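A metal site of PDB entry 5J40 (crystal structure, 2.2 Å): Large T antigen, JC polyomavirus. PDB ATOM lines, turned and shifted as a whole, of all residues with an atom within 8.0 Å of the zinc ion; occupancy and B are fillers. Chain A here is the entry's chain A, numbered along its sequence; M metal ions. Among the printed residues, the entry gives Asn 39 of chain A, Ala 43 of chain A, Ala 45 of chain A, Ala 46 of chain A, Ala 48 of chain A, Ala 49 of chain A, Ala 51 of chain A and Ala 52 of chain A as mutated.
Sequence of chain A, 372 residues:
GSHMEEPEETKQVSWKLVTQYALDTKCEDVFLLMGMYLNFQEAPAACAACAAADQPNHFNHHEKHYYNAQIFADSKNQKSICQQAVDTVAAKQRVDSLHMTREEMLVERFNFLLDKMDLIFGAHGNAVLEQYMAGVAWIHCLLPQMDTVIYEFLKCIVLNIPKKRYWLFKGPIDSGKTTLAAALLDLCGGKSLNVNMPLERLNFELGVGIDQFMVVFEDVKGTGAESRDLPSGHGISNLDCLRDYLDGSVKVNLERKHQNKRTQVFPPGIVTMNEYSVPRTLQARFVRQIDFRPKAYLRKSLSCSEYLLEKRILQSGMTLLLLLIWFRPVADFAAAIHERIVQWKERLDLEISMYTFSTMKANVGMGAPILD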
ATOM      1  N   ASN A  39      19.581  -4.325  36.338  1.00  0.00           N
ATOM      2  CA  ASN A  39      19.006  -3.932  35.038  1.00  0.00           C
ATOM      3  C   ASN A  39      17.792  -4.754  34.588  1.00  0.00           C
ATOM      4  O   ASN A  39      17.276  -4.486  33.523  1.00  0.00           O
ATOM      5  CB  ASN A  39      20.064  -3.916  33.940  1.00  0.00           C
ATOM      6  CG  ASN A  39      20.934  -2.699  33.996  1.00  0.00           C
ATOM      7  OD1 ASN A  39      20.619  -1.707  34.663  1.00  0.00           O
ATOM      8  ND2 ASN A  39      22.029  -2.749  33.274  1.00  0.00           N
ATOM      9  N   PHE A  40      17.365  -5.753  35.392  1.00  0.00           N
ATOM     10  CA  PHE A  40      16.166  -6.548  35.139  1.00  0.00           C
ATOM     11  C   PHE A  40      14.965  -5.994  35.925  1.00  0.00           C
ATOM     12  O   PHE A  40      13.853  -6.479  35.727  1.00  0.00           O
ATOM     13  CB  PHE A  40      16.380  -8.032  35.499  1.00  0.00           C
ATOM     14  CG  PHE A  40      17.408  -8.804  34.690  1.00  0.00           C
ATOM     15  CD1 PHE A  40      17.528  -8.601  33.318  1.00  0.00           C
ATOM     16  CD2 PHE A  40      18.242  -9.734  35.302  1.00  0.00           C
ATOM     17  CE1 PHE A  40      18.476  -9.310  32.576  1.00  0.00           C
ATOM     18  CE2 PHE A  40      19.198 -10.432  34.558  1.00  0.00           C
ATOM     19  CZ  PHE A  40      19.320 -10.192  33.205  1.00  0.00           C
ATOM     20  N   GLN A  41      15.168  -4.984  36.787  1.00  0.00           N
ATOM     21  CA  GLN A  41      14.135  -4.481  37.694  1.00  0.00           C
ATOM     22  C   GLN A  41      12.962  -3.681  37.044  1.00  0.00           C
ATOM     23  O   GLN A  41      11.920  -3.556  37.674  1.00  0.00           O
ATOM     24  CB  GLN A  41      14.761  -3.677  38.851  1.00  0.00           C
ATOM     25  CG  GLN A  41      15.196  -2.256  38.487  1.00  0.00           C
ATOM     26  CD  GLN A  41      15.682  -1.513  39.707  1.00  0.00           C
ATOM     27  OE1 GLN A  41      16.886  -1.331  39.902  1.00  0.00           O
ATOM     28  NE2 GLN A  41      14.760  -1.053  40.550  1.00  0.00           N
ATOM     29  N   GLU A  42      13.129  -3.115  35.842  1.00  0.00           N
ATOM     30  CA  GLU A  42      12.037  -2.385  35.157  1.00  0.00           C
ATOM     31  C   GLU A  42      11.240  -3.334  34.275  1.00  0.00           C
ATOM     32  O   GLU A  42      11.797  -4.304  33.782  1.00  0.00           O
ATOM     33  CB  GLU A  42      12.561  -1.193  34.335  1.00  0.00           C
ATOM     34  CG  GLU A  42      13.209  -0.092  35.154  1.00  0.00           C
ATOM     35  CD  GLU A  42      12.229   0.807  35.874  1.00  0.00           C
ATOM     36  OE1 GLU A  42      11.784   1.813  35.270  1.00  0.00           O
ATOM     37  OE2 GLU A  42      11.889   0.497  37.045  1.00  0.00           O
ATOM     38  N   ALA A  43       9.930  -3.055  34.069  1.00  0.00           N
ATOM     39  CA  ALA A  43       9.023  -3.896  33.276  1.00  0.00           C
ATOM     40  C   ALA A  43       9.587  -4.320  31.902  1.00  0.00           C
ATOM     41  O   ALA A  43       9.987  -3.442  31.127  1.00  0.00           O
ATOM     42  CB  ALA A  43       7.669  -3.219  33.119  1.00  0.00           C
ATOM     43  N   PRO A  44       9.610  -5.642  31.583  1.00  0.00           N
ATOM     44  CA  PRO A  44      10.132  -6.072  30.268  1.00  0.00           C
ATOM     45  C   PRO A  44       9.325  -5.523  29.092  1.00  0.00           C
ATOM     46  O   PRO A  44       9.913  -5.264  28.054  1.00  0.00           O
ATOM     47  CB  PRO A  44      10.058  -7.605  30.347  1.00  0.00           C
ATOM     48  CG  PRO A  44       9.988  -7.922  31.817  1.00  0.00           C
ATOM     49  CD  PRO A  44       9.182  -6.805  32.385  1.00  0.00           C
ATOM     50  N   ALA A  45       7.996  -5.298  29.287  1.00  0.00           N
ATOM     51  CA  ALA A  45       7.090  -4.774  28.243  1.00  0.00           C
ATOM     52  C   ALA A  45       7.538  -3.433  27.648  1.00  0.00           C
ATOM     53  O   ALA A  45       7.384  -3.218  26.441  1.00  0.00           O
ATOM     54  CB  ALA A  45       5.673  -4.673  28.774  1.00  0.00           C
ATOM     55  N   ALA A  46       8.102  -2.546  28.486  1.00  0.00           N
ATOM     56  CA  ALA A  46       8.588  -1.239  28.044  1.00  0.00           C
ATOM     57  C   ALA A  46      10.133  -1.172  28.048  1.00  0.00           C
ATOM     58  O   ALA A  46      10.723  -0.081  28.022  1.00  0.00           O
ATOM     59  CB  ALA A  46       7.984  -0.130  28.904  1.00  0.00           C
ATOM     60  N   CYS A  47      10.799  -2.345  28.048  1.00  0.00           N
ATOM     61  CA  CYS A  47      12.267  -2.381  28.037  1.00  0.00           C
ATOM     62  C   CYS A  47      12.851  -2.154  26.654  1.00  0.00           C
ATOM     63  O   CYS A  47      12.622  -2.947  25.739  1.00  0.00           O
ATOM     64  CB  CYS A  47      12.812  -3.658  28.675  1.00  0.00           C
ATOM     65  SG  CYS A  47      14.618  -3.699  28.795  1.00  0.00           S
ATOM     66  N   ALA A  48      13.624  -1.060  26.514  1.00  0.00           N
ATOM     67  CA  ALA A  48      14.295  -0.707  25.267  1.00  0.00           C
ATOM     68  C   ALA A  48      15.410  -1.713  24.942  1.00  0.00           C
ATOM     69  O   ALA A  48      15.618  -2.036  23.773  1.00  0.00           O
ATOM     70  CB  ALA A  48      14.865   0.704  25.362  1.00  0.00           C
ATOM     71  N   ALA A  49      16.116  -2.230  25.967  1.00  0.00           N
ATOM     72  CA  ALA A  49      17.199  -3.206  25.771  1.00  0.00           C
ATOM     73  C   ALA A  49      16.659  -4.525  25.202  1.00  0.00           C
ATOM     74  O   ALA A  49      17.279  -5.076  24.293  1.00  0.00           O
ATOM     75  CB  ALA A  49      17.946  -3.437  27.072  1.00  0.00           C
ATOM     76  N   CYS A  50      15.479  -4.998  25.680  1.00  0.00           N
ATOM     77  CA  CYS A  50      14.837  -6.200  25.165  1.00  0.00           C
ATOM     78  C   CYS A  50      14.402  -5.973  23.719  1.00  0.00           C
ATOM     79  O   CYS A  50      14.580  -6.860  22.888  1.00  0.00           O
ATOM     80  CB  CYS A  50      13.654  -6.622  26.038  1.00  0.00           C
ATOM     81  SG  CYS A  50      14.138  -7.447  27.586  1.00  0.00           S
ATOM     82  N   ALA A  51      13.884  -4.756  23.430  1.00  0.00           N
ATOM     83  CA  ALA A  51      13.432  -4.311  22.104  1.00  0.00           C
ATOM     84  C   ALA A  51      14.579  -4.268  21.086  1.00  0.00           C
ATOM     85  O   ALA A  51      14.398  -4.710  19.954  1.00  0.00           O
ATOM     86  CB  ALA A  51      12.751  -2.948  22.217  1.00  0.00           C
ATOM     87  N   ALA A  52      15.772  -3.780  21.505  1.00  0.00           N
ATOM     88  CA  ALA A  52      16.990  -3.711  20.694  1.00  0.00           C
ATOM     89  C   ALA A  52      17.554  -5.125  20.386  1.00  0.00           C
ATOM     90  O   ALA A  52      18.202  -5.308  19.360  1.00  0.00           O
ATOM     91  CB  ALA A  52      18.050  -2.875  21.404  1.00  0.00           C
ATOM     92  N   GLN A  55      21.892  -7.749  23.359  1.00  0.00           N
ATOM     93  CA  GLN A  55      22.671  -8.280  24.495  1.00  0.00           C
ATOM     94  C   GLN A  55      21.957  -9.497  25.078  1.00  0.00           C
ATOM     95  O   GLN A  55      21.085  -9.323  25.927  1.00  0.00           O
ATOM     96  CB  GLN A  55      22.971  -7.185  25.536  1.00  0.00           C
ATOM     97  CG  GLN A  55      24.240  -7.461  26.339  1.00  0.00           C
ATOM     98  CD  GLN A  55      24.524  -6.490  27.469  1.00  0.00           C
ATOM     99  OE1 GLN A  55      23.654  -5.734  27.940  1.00  0.00           O
ATOM    100  NE2 GLN A  55      25.748  -6.523  27.970  1.00  0.00           N
ATOM    101  N   HIS A  58      21.086 -10.119  28.666  1.00  0.00           N
ATOM    102  CA  HIS A  58      19.992  -9.306  29.160  1.00  0.00           C
ATOM    103  C   HIS A  58      18.642  -9.837  28.673  1.00  0.00           C
ATOM    104  O   HIS A  58      17.824 -10.241  29.495  1.00  0.00           O
ATOM    105  CB  HIS A  58      20.136  -7.821  28.814  1.00  0.00           C
ATOM    106  CG  HIS A  58      18.926  -7.054  29.266  1.00  0.00           C
ATOM    107  ND1 HIS A  58      18.819  -6.562  30.564  1.00  0.00           N
ATOM    108  CD2 HIS A  58      17.741  -6.875  28.628  1.00  0.00           C
ATOM    109  CE1 HIS A  58      17.604  -6.048  30.646  1.00  0.00           C
ATOM    110  NE2 HIS A  58      16.918  -6.225  29.517  1.00  0.00           N
ATOM    111  N   PHE A  59      18.396  -9.771  27.337  1.00  0.00           N
ATOM    112  CA  PHE A  59      17.102 -10.070  26.704  1.00  0.00           C
ATOM    113  C   PHE A  59      16.605 -11.526  26.855  1.00  0.00           C
ATOM    114  O   PHE A  59      15.385 -11.747  26.779  1.00  0.00           O
ATOM    115  CB  PHE A  59      17.073  -9.619  25.214  1.00  0.00           C
ATOM    116  CG  PHE A  59      17.795 -10.441  24.163  1.00  0.00           C
ATOM    117  CD1 PHE A  59      17.253 -11.614  23.670  1.00  0.00           C
ATOM    118  CD2 PHE A  59      18.944  -9.949  23.548  1.00  0.00           C
ATOM    119  CE1 PHE A  59      17.905 -12.347  22.665  1.00  0.00           C
ATOM    120  CE2 PHE A  59      19.579 -10.669  22.531  1.00  0.00           C
ATOM    121  CZ  PHE A  59      19.063 -11.865  22.100  1.00  0.00           C
ATOM    122  N   ASN A  60      17.502 -12.498  27.093  1.00  0.00           N
ATOM    123  CA  ASN A  60      17.050 -13.887  27.274  1.00  0.00           C
ATOM    124  C   ASN A  60      16.708 -14.222  28.726  1.00  0.00           C
ATOM    125  O   ASN A  60      16.135 -15.281  29.014  1.00  0.00           O
ATOM    126  CB  ASN A  60      18.074 -14.870  26.705  1.00  0.00           C
ATOM    127  CG  ASN A  60      17.993 -14.964  25.205  1.00  0.00           C
ATOM    128  OD1 ASN A  60      16.922 -15.139  24.610  1.00  0.00           O
ATOM    129  ND2 ASN A  60      19.132 -14.842  24.547  1.00  0.00           N
ATOM    130  N   HIS A  61      16.999 -13.289  29.625  1.00  0.00           N
ATOM    131  CA  HIS A  61      16.820 -13.485  31.043  1.00  0.00           C
ATOM    132  C   HIS A  61      15.890 -12.466  31.737  1.00  0.00           C
ATOM    133  O   HIS A  61      15.401 -12.753  32.829  1.00  0.00           O
ATOM    134  CB  HIS A  61      18.193 -13.521  31.716  1.00  0.00           C
ATOM    135  CG  HIS A  61      19.123 -14.507  31.095  1.00  0.00           C
ATOM    136  ND1 HIS A  61      19.093 -15.856  31.449  1.00  0.00           N
ATOM    137  CD2 HIS A  61      20.059 -14.333  30.133  1.00  0.00           C
ATOM    138  CE1 HIS A  61      20.008 -16.440  30.691  1.00  0.00           C
ATOM    139  NE2 HIS A  61      20.625 -15.568  29.895  1.00  0.00           N
ATOM    140  N   HIS A  62      15.620 -11.312  31.107  1.00  0.00           N
ATOM    141  CA  HIS A  62      14.812 -10.245  31.709  1.00  0.00           C
ATOM    142  C   HIS A  62      13.445 -10.709  32.207  1.00  0.00           C
ATOM    143  O   HIS A  62      13.115 -10.436  33.347  1.00  0.00           O
ATOM    144  CB  HIS A  62      14.674  -9.020  30.759  1.00  0.00           C
ATOM    145  CG  HIS A  62      14.237  -7.746  31.425  1.00  0.00           C
ATOM    146  ND1 HIS A  62      14.293  -6.531  30.769  1.00  0.00           N
ATOM    147  CD2 HIS A  62      13.762  -7.536  32.674  1.00  0.00           C
ATOM    148  CE1 HIS A  62      13.843  -5.630  31.622  1.00  0.00           C
ATOM    149  NE2 HIS A  62      13.497  -6.183  32.776  1.00  0.00           N
ATOM    150  N   GLU A  63      12.673 -11.435  31.386  1.00  0.00           N
ATOM    151  CA  GLU A  63      11.342 -11.912  31.769  1.00  0.00           C
ATOM    152  C   GLU A  63      11.362 -12.870  32.965  1.00  0.00           C
ATOM    153  O   GLU A  63      10.542 -12.697  33.870  1.00  0.00           O
ATOM    154  CB  GLU A  63      10.604 -12.538  30.573  1.00  0.00           C
ATOM    155  CG  GLU A  63       9.108 -12.633  30.786  1.00  0.00           C
ATOM    156  CD  GLU A  63       8.364 -11.330  30.526  1.00  0.00           C
ATOM    157  OE1 GLU A  63       8.120 -11.012  29.344  1.00  0.00           O
ATOM    158  OE2 GLU A  63       8.024 -10.642  31.520  1.00  0.00           O
HETATM  159 ZN    ZN M   1      14.959  -6.003  29.037  1.00  0.00          ZN
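A ring nitrogen (NE2) of His 62 lies within hydrogen-bond range of the backbone carbonyl oxygen (O) of Phe 40, at 3.0 Å.
NE2 of His 62 sits at hydrogen-bond distance from O of Glu 42 (2.7 Å).
SG of Cys 47 lies close to N of Ala 49 (3.5 Å).
Four residues have an atom within 4 Å of the zinc ion: Cys 47, Cys 50, His 58 and His 62.
Along chain A the residues within 4 Å of the zinc ion span positions 47 to 62.
The nearest printed residue that does not touch the zinc ion is Ala 49 (4.4 Å).
The zinc ion is bound by a ring nitrogen (ND1) of His 62, a ring nitrogen (NE2) of His 58, the side-chain sulfur (SG) of Cys 50 and the side-chain sulfur (SG) of Cys 47.
The zinc ion has four donor atoms within binding distance.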
